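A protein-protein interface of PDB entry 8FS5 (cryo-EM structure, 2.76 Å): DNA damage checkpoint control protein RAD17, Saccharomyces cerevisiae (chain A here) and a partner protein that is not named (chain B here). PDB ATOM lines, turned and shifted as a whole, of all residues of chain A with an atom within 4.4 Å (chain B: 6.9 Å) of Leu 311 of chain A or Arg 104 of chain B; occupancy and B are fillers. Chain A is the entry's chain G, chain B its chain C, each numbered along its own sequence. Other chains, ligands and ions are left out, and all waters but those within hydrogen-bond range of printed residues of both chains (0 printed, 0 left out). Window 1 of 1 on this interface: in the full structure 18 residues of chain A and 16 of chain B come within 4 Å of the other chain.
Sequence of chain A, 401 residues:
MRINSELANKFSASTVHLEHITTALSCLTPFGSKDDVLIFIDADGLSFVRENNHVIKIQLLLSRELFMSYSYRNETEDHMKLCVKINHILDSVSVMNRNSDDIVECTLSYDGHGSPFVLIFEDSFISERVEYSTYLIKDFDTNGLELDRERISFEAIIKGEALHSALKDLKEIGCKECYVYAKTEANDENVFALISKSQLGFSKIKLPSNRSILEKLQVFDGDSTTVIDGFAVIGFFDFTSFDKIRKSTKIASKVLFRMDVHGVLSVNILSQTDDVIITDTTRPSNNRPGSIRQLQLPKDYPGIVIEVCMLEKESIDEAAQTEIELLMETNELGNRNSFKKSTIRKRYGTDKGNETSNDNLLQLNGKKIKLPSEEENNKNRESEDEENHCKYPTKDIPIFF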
ATOM      1  N   HIS A  54      -1.089 -23.519  -7.696  1.00  0.00           N
ATOM      2  CA  HIS A  54      -1.636 -22.170  -7.556  1.00  0.00           C
ATOM      3  C   HIS A  54      -0.562 -21.088  -7.586  1.00  0.00           C
ATOM      4  O   HIS A  54      -0.788 -19.979  -7.092  1.00  0.00           O
ATOM      5  CB  HIS A  54      -2.475 -22.018  -6.277  1.00  0.00           C
ATOM      6  CG  HIS A  54      -3.570 -23.030  -6.131  1.00  0.00           C
ATOM      7  ND1 HIS A  54      -3.341 -24.389  -6.137  1.00  0.00           N
ATOM      8  CD2 HIS A  54      -4.905 -22.875  -5.965  1.00  0.00           C
ATOM      9  CE1 HIS A  54      -4.488 -25.028  -5.986  1.00  0.00           C
ATOM     10  NE2 HIS A  54      -5.451 -24.132  -5.879  1.00  0.00           N
ATOM     11  N   VAL A  55       0.609 -21.380  -8.153  1.00  0.00           N
ATOM     12  CA  VAL A  55       1.716 -20.430  -8.154  1.00  0.00           C
ATOM     13  C   VAL A  55       2.115 -20.095  -9.585  1.00  0.00           C
ATOM     14  O   VAL A  55       2.755 -19.069  -9.838  1.00  0.00           O
ATOM     15  CB  VAL A  55       2.920 -20.974  -7.362  1.00  0.00           C
ATOM     16  CG1 VAL A  55       2.551 -21.162  -5.901  1.00  0.00           C
ATOM     17  CG2 VAL A  55       3.410 -22.280  -7.964  1.00  0.00           C
ATOM     18  N   LEU A 145      -4.585 -15.774 -11.354  1.00  0.00           N
ATOM     19  CA  LEU A 145      -3.143 -15.683 -11.588  1.00  0.00           C
ATOM     20  C   LEU A 145      -2.887 -14.920 -12.885  1.00  0.00           C
ATOM     21  O   LEU A 145      -2.365 -15.449 -13.868  1.00  0.00           O
ATOM     22  CB  LEU A 145      -2.519 -17.071 -11.625  1.00  0.00           C
ATOM     23  CG  LEU A 145      -1.452 -17.363 -10.571  1.00  0.00           C
ATOM     24  CD1 LEU A 145      -0.863 -18.743 -10.791  1.00  0.00           C
ATOM     25  CD2 LEU A 145      -0.364 -16.300 -10.598  1.00  0.00           C
ATOM     26  N   PHE A 237      12.246 -15.290  -7.767  1.00  0.00           N
ATOM     27  CA  PHE A 237      11.453 -16.387  -8.298  1.00  0.00           C
ATOM     28  C   PHE A 237      12.129 -17.714  -7.989  1.00  0.00           C
ATOM     29  O   PHE A 237      13.353 -17.801  -7.862  1.00  0.00           O
ATOM     30  CB  PHE A 237      11.251 -16.255  -9.814  1.00  0.00           C
ATOM     31  CG  PHE A 237      10.466 -15.043 -10.218  1.00  0.00           C
ATOM     32  CD1 PHE A 237       9.086 -15.026 -10.107  1.00  0.00           C
ATOM     33  CD2 PHE A 237      11.108 -13.921 -10.713  1.00  0.00           C
ATOM     34  CE1 PHE A 237       8.361 -13.913 -10.478  1.00  0.00           C
ATOM     35  CE2 PHE A 237      10.389 -12.803 -11.087  1.00  0.00           C
ATOM     36  CZ  PHE A 237       9.014 -12.800 -10.969  1.00  0.00           C
ATOM     37  N   VAL A 261       3.624  -4.657  -9.462  1.00  0.00           N
ATOM     38  CA  VAL A 261       4.039  -4.504  -8.069  1.00  0.00           C
ATOM     39  C   VAL A 261       3.498  -5.601  -7.169  1.00  0.00           C
ATOM     40  O   VAL A 261       3.925  -5.706  -6.013  1.00  0.00           O
ATOM     41  CB  VAL A 261       3.602  -3.138  -7.509  1.00  0.00           C
ATOM     42  CG1 VAL A 261       4.594  -2.058  -7.912  1.00  0.00           C
ATOM     43  CG2 VAL A 261       2.202  -2.791  -7.988  1.00  0.00           C
ATOM     44  N   HIS A 262       2.572  -6.420  -7.663  1.00  0.00           N
ATOM     45  CA  HIS A 262       2.012  -7.516  -6.882  1.00  0.00           C
ATOM     46  C   HIS A 262       2.860  -8.779  -6.941  1.00  0.00           C
ATOM     47  O   HIS A 262       2.510  -9.771  -6.292  1.00  0.00           O
ATOM     48  CB  HIS A 262       0.590  -7.825  -7.361  1.00  0.00           C
ATOM     49  CG  HIS A 262      -0.292  -6.619  -7.453  1.00  0.00           C
ATOM     50  ND1 HIS A 262      -0.895  -6.052  -6.351  1.00  0.00           N
ATOM     51  CD2 HIS A 262      -0.671  -5.871  -8.516  1.00  0.00           C
ATOM     52  CE1 HIS A 262      -1.609  -5.007  -6.732  1.00  0.00           C
ATOM     53  NE2 HIS A 262      -1.490  -4.876  -8.040  1.00  0.00           N
ATOM     54  N   GLY A 263       3.957  -8.768  -7.694  1.00  0.00           N
ATOM     55  CA  GLY A 263       4.842  -9.913  -7.771  1.00  0.00           C
ATOM     56  C   GLY A 263       4.355 -11.004  -8.702  1.00  0.00           C
ATOM     57  O   GLY A 263       4.388 -12.187  -8.351  1.00  0.00           O
ATOM     58  N   VAL A 264       3.900 -10.621  -9.894  1.00  0.00           N
ATOM     59  CA  VAL A 264       3.445 -11.572 -10.903  1.00  0.00           C
ATOM     60  C   VAL A 264       4.196 -11.288 -12.196  1.00  0.00           C
ATOM     61  O   VAL A 264       4.151 -10.164 -12.709  1.00  0.00           O
ATOM     62  CB  VAL A 264       1.926 -11.493 -11.141  1.00  0.00           C
ATOM     63  CG1 VAL A 264       1.517 -12.437 -12.263  1.00  0.00           C
ATOM     64  CG2 VAL A 264       1.174 -11.829  -9.867  1.00  0.00           C
ATOM     65  N   MET A 310       3.517 -16.243 -13.488  1.00  0.00           N
ATOM     66  CA  MET A 310       4.315 -16.806 -12.408  1.00  0.00           C
ATOM     67  C   MET A 310       4.265 -15.891 -11.196  1.00  0.00           C
ATOM     68  O   MET A 310       4.277 -14.666 -11.339  1.00  0.00           O
ATOM     69  CB  MET A 310       5.765 -17.009 -12.857  1.00  0.00           C
ATOM     70  CG  MET A 310       6.553 -18.000 -12.025  1.00  0.00           C
ATOM     71  SD  MET A 310       8.258 -18.168 -12.590  1.00  0.00           S
ATOM     72  CE  MET A 310       8.146 -17.505 -14.252  1.00  0.00           C
ATOM     73  N   LEU A 311       4.212 -16.488 -10.009  1.00  0.00           N
ATOM     74  CA  LEU A 311       4.189 -15.725  -8.770  1.00  0.00           C
ATOM     75  C   LEU A 311       5.598 -15.574  -8.206  1.00  0.00           C
ATOM     76  O   LEU A 311       6.489 -16.387  -8.468  1.00  0.00           O
ATOM     77  CB  LEU A 311       3.282 -16.399  -7.741  1.00  0.00           C
ATOM     78  CG  LEU A 311       1.878 -15.806  -7.599  1.00  0.00           C
ATOM     79  CD1 LEU A 311       1.020 -16.664  -6.684  1.00  0.00           C
ATOM     80  CD2 LEU A 311       1.945 -14.374  -7.088  1.00  0.00           C
ATOM     81  N   GLU A 312       5.791 -14.518  -7.422  1.00  0.00           N
ATOM     82  CA  GLU A 312       7.092 -14.176  -6.868  1.00  0.00           C
ATOM     83  C   GLU A 312       7.141 -14.517  -5.380  1.00  0.00           C
ATOM     84  O   GLU A 312       6.146 -14.392  -4.662  1.00  0.00           O
ATOM     85  CB  GLU A 312       7.392 -12.690  -7.101  1.00  0.00           C
ATOM     86  CG  GLU A 312       8.361 -12.043  -6.124  1.00  0.00           C
ATOM     87  CD  GLU A 312       8.753 -10.641  -6.543  1.00  0.00           C
ATOM     88  OE1 GLU A 312       8.271 -10.180  -7.599  1.00  0.00           O
ATOM     89  OE2 GLU A 312       9.543 -10.000  -5.819  1.00  0.00           O
ATOM     90  N   LYS A 313       8.310 -14.969  -4.931  1.00  0.00           N
ATOM     91  CA  LYS A 313       8.490 -15.406  -3.554  1.00  0.00           C
ATOM     92  C   LYS A 313       8.430 -14.225  -2.584  1.00  0.00           C
ATOM     93  O   LYS A 313       8.463 -13.055  -2.977  1.00  0.00           O
ATOM     94  CB  LYS A 313       9.823 -16.139  -3.401  1.00  0.00           C
ATOM     95  CG  LYS A 313       9.997 -17.314  -4.349  1.00  0.00           C
ATOM     96  CD  LYS A 313       9.781 -18.641  -3.643  1.00  0.00           C
ATOM     97  CE  LYS A 313      10.854 -18.886  -2.595  1.00  0.00           C
ATOM     98  NZ  LYS A 313      12.219 -18.834  -3.188  1.00  0.00           N
ATOM     99  N   GLU A 314       8.332 -14.556  -1.292  1.00  0.00           N
ATOM    100  CA  GLU A 314       8.276 -13.536  -0.248  1.00  0.00           C
ATOM    101  C   GLU A 314       9.562 -12.722  -0.176  1.00  0.00           C
ATOM    102  O   GLU A 314       9.513 -11.496  -0.016  1.00  0.00           O
ATOM    103  CB  GLU A 314       8.007 -14.182   1.111  1.00  0.00           C
ATOM    104  CG  GLU A 314       6.560 -14.521   1.409  1.00  0.00           C
ATOM    105  CD  GLU A 314       5.576 -13.660   0.649  1.00  0.00           C
ATOM    106  OE1 GLU A 314       5.215 -12.578   1.160  1.00  0.00           O
ATOM    107  OE2 GLU A 314       5.143 -14.074  -0.444  1.00  0.00           O
ATOM    108  N   ASN B  77      -8.131 -18.905  -5.321  1.00  0.00           N
ATOM    109  CA  ASN B  77      -6.688 -18.739  -5.432  1.00  0.00           C
ATOM    110  C   ASN B  77      -5.994 -18.472  -4.104  1.00  0.00           C
ATOM    111  O   ASN B  77      -4.760 -18.398  -4.079  1.00  0.00           O
ATOM    112  CB  ASN B  77      -6.354 -17.595  -6.397  1.00  0.00           C
ATOM    113  CG  ASN B  77      -5.223 -17.943  -7.347  1.00  0.00           C
ATOM    114  OD1 ASN B  77      -5.197 -19.027  -7.930  1.00  0.00           O
ATOM    115  ND2 ASN B  77      -4.275 -17.027  -7.498  1.00  0.00           N
ATOM    116  N   MET B  78      -6.737 -18.324  -3.011  1.00  0.00           N
ATOM    117  CA  MET B  78      -6.141 -17.937  -1.740  1.00  0.00           C
ATOM    118  C   MET B  78      -6.205 -19.038  -0.693  1.00  0.00           C
ATOM    119  O   MET B  78      -5.630 -18.880   0.389  1.00  0.00           O
ATOM    120  CB  MET B  78      -6.827 -16.682  -1.196  1.00  0.00           C
ATOM    121  CG  MET B  78      -6.350 -15.352  -1.787  1.00  0.00           C
ATOM    122  SD  MET B  78      -4.837 -14.627  -1.115  1.00  0.00           S
ATOM    123  CE  MET B  78      -3.568 -15.608  -1.915  1.00  0.00           C
ATOM    124  N   ASP B  99       5.781 -24.179  -1.614  1.00  0.00           N
ATOM    125  CA  ASP B  99       5.681 -23.167  -2.661  1.00  0.00           C
ATOM    126  C   ASP B  99       4.378 -22.381  -2.586  1.00  0.00           C
ATOM    127  O   ASP B  99       4.344 -21.221  -3.012  1.00  0.00           O
ATOM    128  CB  ASP B  99       5.842 -23.791  -4.050  1.00  0.00           C
ATOM    129  CG  ASP B  99       7.001 -24.762  -4.122  1.00  0.00           C
ATOM    130  OD1 ASP B  99       7.775 -24.839  -3.146  1.00  0.00           O
ATOM    131  OD2 ASP B  99       7.140 -25.448  -5.157  1.00  0.00           O
ATOM    132  N   PHE B 100       3.299 -22.971  -2.065  1.00  0.00           N
ATOM    133  CA  PHE B 100       2.104 -22.176  -1.820  1.00  0.00           C
ATOM    134  C   PHE B 100       2.318 -21.136  -0.730  1.00  0.00           C
ATOM    135  O   PHE B 100       1.828 -20.010  -0.861  1.00  0.00           O
ATOM    136  CB  PHE B 100       0.922 -23.075  -1.450  1.00  0.00           C
ATOM    137  CG  PHE B 100      -0.384 -22.338  -1.328  1.00  0.00           C
ATOM    138  CD1 PHE B 100      -1.132 -22.036  -2.454  1.00  0.00           C
ATOM    139  CD2 PHE B 100      -0.862 -21.946  -0.088  1.00  0.00           C
ATOM    140  CE1 PHE B 100      -2.331 -21.358  -2.346  1.00  0.00           C
ATOM    141  CE2 PHE B 100      -2.061 -21.267   0.026  1.00  0.00           C
ATOM    142  CZ  PHE B 100      -2.796 -20.973  -1.103  1.00  0.00           C
ATOM    143  N   ALA B 101       3.042 -21.485   0.333  1.00  0.00           N
ATOM    144  CA  ALA B 101       3.320 -20.542   1.408  1.00  0.00           C
ATOM    145  C   ALA B 101       4.378 -19.511   1.039  1.00  0.00           C
ATOM    146  O   ALA B 101       4.298 -18.365   1.494  1.00  0.00           O
ATOM    147  CB  ALA B 101       3.759 -21.293   2.666  1.00  0.00           C
ATOM    148  N   SER B 102       5.368 -19.887   0.226  1.00  0.00           N
ATOM    149  CA  SER B 102       6.477 -18.987  -0.073  1.00  0.00           C
ATOM    150  C   SER B 102       6.102 -17.898  -1.072  1.00  0.00           C
ATOM    151  O   SER B 102       6.591 -16.769  -0.957  1.00  0.00           O
ATOM    152  CB  SER B 102       7.669 -19.787  -0.601  1.00  0.00           C
ATOM    153  OG  SER B 102       7.962 -20.882   0.249  1.00  0.00           O
ATOM    154  N   THR B 103       5.256 -18.209  -2.050  1.00  0.00           N
ATOM    155  CA  THR B 103       4.924 -17.242  -3.085  1.00  0.00           C
ATOM    156  C   THR B 103       4.005 -16.151  -2.538  1.00  0.00           C
ATOM    157  O   THR B 103       3.404 -16.282  -1.469  1.00  0.00           O
ATOM    158  CB  THR B 103       4.261 -17.935  -4.276  1.00  0.00           C
ATOM    159  OG1 THR B 103       3.175 -18.745  -3.813  1.00  0.00           O
ATOM    160  CG2 THR B 103       5.269 -18.807  -5.010  1.00  0.00           C
ATOM    161  N   ARG B 104       3.900 -15.062  -3.297  1.00  0.00           N
ATOM    162  CA  ARG B 104       3.115 -13.917  -2.864  1.00  0.00           C
ATOM    163  C   ARG B 104       1.624 -14.163  -3.073  1.00  0.00           C
ATOM    164  O   ARG B 104       1.199 -15.120  -3.727  1.00  0.00           O
ATOM    165  CB  ARG B 104       3.555 -12.647  -3.593  1.00  0.00           C
ATOM    166  CG  ARG B 104       4.800 -11.999  -3.005  1.00  0.00           C
ATOM    167  CD  ARG B 104       5.510 -11.120  -4.019  1.00  0.00           C
ATOM    168  NE  ARG B 104       5.094  -9.726  -3.915  1.00  0.00           N
ATOM    169  CZ  ARG B 104       5.889  -8.688  -4.139  1.00  0.00           C
ATOM    170  NH1 ARG B 104       7.160  -8.847  -4.469  1.00  0.00           N
ATOM    171  NH2 ARG B 104       5.395  -7.457  -4.028  1.00  0.00           N
ATOM    172  N   GLN B 105       0.824 -13.267  -2.499  1.00  0.00           N
ATOM    173  CA  GLN B 105      -0.628 -13.374  -2.480  1.00  0.00           C
ATOM    174  C   GLN B 105      -1.284 -12.393  -3.445  1.00  0.00           C
ATOM    175  O   GLN B 105      -2.452 -12.039  -3.269  1.00  0.00           O
ATOM    176  CB  GLN B 105      -1.155 -13.149  -1.063  1.00  0.00           C
ATOM    177  CG  GLN B 105      -0.609 -11.904  -0.376  1.00  0.00           C
ATOM    178  CD  GLN B 105       0.697 -12.156   0.355  1.00  0.00           C
ATOM    179  OE1 GLN B 105       0.804 -13.082   1.158  1.00  0.00           O
ATOM    180  NE2 GLN B 105       1.699 -11.329   0.077  1.00  0.00           N
ATOM    181  N   ILE B 106      -0.522 -11.925  -4.443  1.00  0.00           N
ATOM    182  CA  ILE B 106      -0.899 -10.914  -5.438  1.00  0.00           C
ATOM    183  C   ILE B 106      -1.558  -9.702  -4.772  1.00  0.00           C
ATOM    184  O   ILE B 106      -2.288  -8.937  -5.414  1.00  0.00           O
ATOM    185  CB  ILE B 106      -1.765 -11.536  -6.564  1.00  0.00           C
ATOM    186  CG1 ILE B 106      -1.646 -10.721  -7.860  1.00  0.00           C
ATOM    187  CG2 ILE B 106      -3.239 -11.721  -6.182  1.00  0.00           C
ATOM    188  CD1 ILE B 106      -2.506 -11.240  -8.993  1.00  0.00           C
ATOM    189  N   PHE B 107      -1.232  -9.483  -3.499  1.00  0.00           N
ATOM    190  CA  PHE B 107      -1.750  -8.377  -2.693  1.00  0.00           C
ATOM    191  C   PHE B 107      -3.278  -8.348  -2.719  1.00  0.00           C
ATOM    192  O   PHE B 107      -3.911  -7.312  -2.930  1.00  0.00           O
ATOM    193  CB  PHE B 107      -1.166  -7.038  -3.147  1.00  0.00           C
ATOM    194  CG  PHE B 107       0.251  -6.795  -2.688  1.00  0.00           C
ATOM    195  CD1 PHE B 107       1.224  -7.775  -2.812  1.00  0.00           C
ATOM    196  CD2 PHE B 107       0.607  -5.576  -2.132  1.00  0.00           C
ATOM    197  CE1 PHE B 107       2.520  -7.547  -2.390  1.00  0.00           C
ATOM    198  CE2 PHE B 107       1.902  -5.342  -1.709  1.00  0.00           C
ATOM    199  CZ  PHE B 107       2.860  -6.327  -1.838  1.00  0.00           C
ATOM    200  N   LYS B 112      -2.364 -15.910   3.286  1.00  0.00           N
ATOM    201  CA  LYS B 112      -2.907 -17.126   2.704  1.00  0.00           C
ATOM    202  C   LYS B 112      -3.428 -18.056   3.797  1.00  0.00           C
ATOM    203  O   LYS B 112      -3.095 -17.922   4.976  1.00  0.00           O
ATOM    204  CB  LYS B 112      -1.845 -17.835   1.863  1.00  0.00           C
ATOM    205  CG  LYS B 112      -1.486 -17.105   0.585  1.00  0.00           C
ATOM    206  CD  LYS B 112      -0.234 -17.678  -0.049  1.00  0.00           C
ATOM    207  CE  LYS B 112      -0.207 -17.415  -1.546  1.00  0.00           C
ATOM    208  NZ  LYS B 112       0.831 -18.230  -2.235  1.00  0.00           N
ATOM    209  N   ASN B 140       2.725 -14.587   5.897  1.00  0.00           N
ATOM    210  CA  ASN B 140       1.911 -14.583   4.692  1.00  0.00           C
ATOM    211  C   ASN B 140       0.918 -15.732   4.607  1.00  0.00           C
ATOM    212  O   ASN B 140       0.057 -15.709   3.720  1.00  0.00           O
ATOM    213  CB  ASN B 140       2.801 -14.630   3.442  1.00  0.00           C
ATOM    214  CG  ASN B 140       3.982 -15.559   3.611  1.00  0.00           C
ATOM    215  OD1 ASN B 140       4.649 -15.552   4.645  1.00  0.00           O
ATOM    216  ND2 ASN B 140       4.222 -16.396   2.612  1.00  0.00           N
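The side-chain hydroxyl (OG1) of Thr 103 of chain B sits at hydrogen-bond distance from the backbone carbonyl oxygen (O) of Asp 99 of chain B (2.9 Å).
The backbone carbonyl oxygen (O) of Phe 100 of chain B is in hydrogen-bond range of the side-chain hydroxyl (OG1) of Thr 103 of chain B (3.5 Å).
The backbone carbonyl oxygen (O) of Phe 100 of chain B sits at hydrogen-bond distance from the side-chain amino group (NZ) of Lys 112 of chain B (2.5 Å).
OG1 of Thr 103 of chain B lies within hydrogen-bond range of NZ of Lys 112 of chain B (2.9 Å).
The side-chain amino group of Lys 112 of chain B lies close to the backbone carbonyl oxygen of Arg 104 of chain B (3.5 Å).
The backbone carbonyl oxygen of Gly 263 of chain A sits at hydrogen-bond distance from the backbone NH of Glu 312 of chain A (2.9 Å).
O of Ser 102 of chain B lies within hydrogen-bond range of N of Glu 314 of chain A (2.8 Å).
The guanidinium group of Arg 104 of chain B is in hydrogen-bond range of the backbone carbonyl oxygen of Val 261 of chain A (3.0 Å).
NH1 of Arg 104 of chain B is in salt-bridge range of OE2 of Glu 312 of chain A, 3.0 Å away.
The backbone NH of Arg 104 of chain B lies close to the side-chain carboxylate of Glu 314 of chain A, at 3.3 Å.
The backbone carbonyl oxygen (O) of Ile 106 of chain B lies within hydrogen-bond range of a ring nitrogen (ND1) of His 262 of chain A (3.3 Å).
The side-chain carboxylate (OE2) of Glu 314 of chain A lies close to the backbone carbonyl oxygen (O) of Thr 103 of chain B (3.0 Å).
Of the 13 printed residues of chain B, 9 touch a printed residue of chain A.
Hydrophobic or aromatic side chains of chain B within 4 Å of the printed part of chain A: Phe 100, Ile 106 and Phe 107.
Printed residues of chain A that touch a printed residue of chain B: His 54, Val 55, Val 261, His 262, Gly 263, Val 264, Leu 311, Glu 312, Lys 313 and Glu 314.
Hydrophobic or aromatic side chains of chain A within 4 Å of the printed part of chain B: His 54, Val 55, His 262, Val 264 and Leu 311.
Among the printed residues, 20 pairs touch across the chains.
Among the printed residues, Asp or Glu carboxylates within 4 Å of a Lys or Arg side-chain nitrogen of the other chain: Glu 312 of chain A with Arg 104 of chain B.
His 54 of chain A touches Phe 100 of chain B.
CG1 of Val 55 of chain A touches O of Asp 99 of chain B, 3.4 Å away.
O of His 262 of chain A touches NE of Arg 104 of chain B (3.5 Å).
His 262 of chain A touches Phe 107 of chain B.
Ile 106 of chain B touches Val 264 of chain A.
CB of Thr 103 of chain B touches CB of Leu 311 of chain A (3.9 Å).
Glu 312 of chain A touches Thr 103 of chain B.
Arg 104 of chain B touches Lys 313 of chain A.
Gln 105 of chain B touches Glu 314 of chain A.
Asn 140 of chain B touches Glu 314 of chain A (ND2 to CG, 3.2 Å).
Leu 311 of chain A touches just these residues of chain B: Thr 103 and Arg 104.
Of chain A, only Val 261 (3.0 Å), His 262 (3.5 Å), Gly 263 (3.9 Å), Leu 311 (3.3 Å), Glu 312 (2.7 Å), Lys 313 (3.7 Å) and Glu 314 (3.2 Å) come within 4 Å of Arg 104 of chain B.
Printed residues of chain B within 4 Å of Val 55 of chain A: Asp 99 and Thr 103.
Of the printed residues of chain A, Phe 100 of chain B touches His 54 (3.99 Å).
Phe 237 of chain A touches none of the printed residues of chain B.
The nearest residue of chain B that does not touch Leu 311 of chain A is Ile 106 of chain B (4.4 Å).
The nearest printed residue of chain B that does not touch His 54 of chain A is Asn 77 of chain B (4.3 Å).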
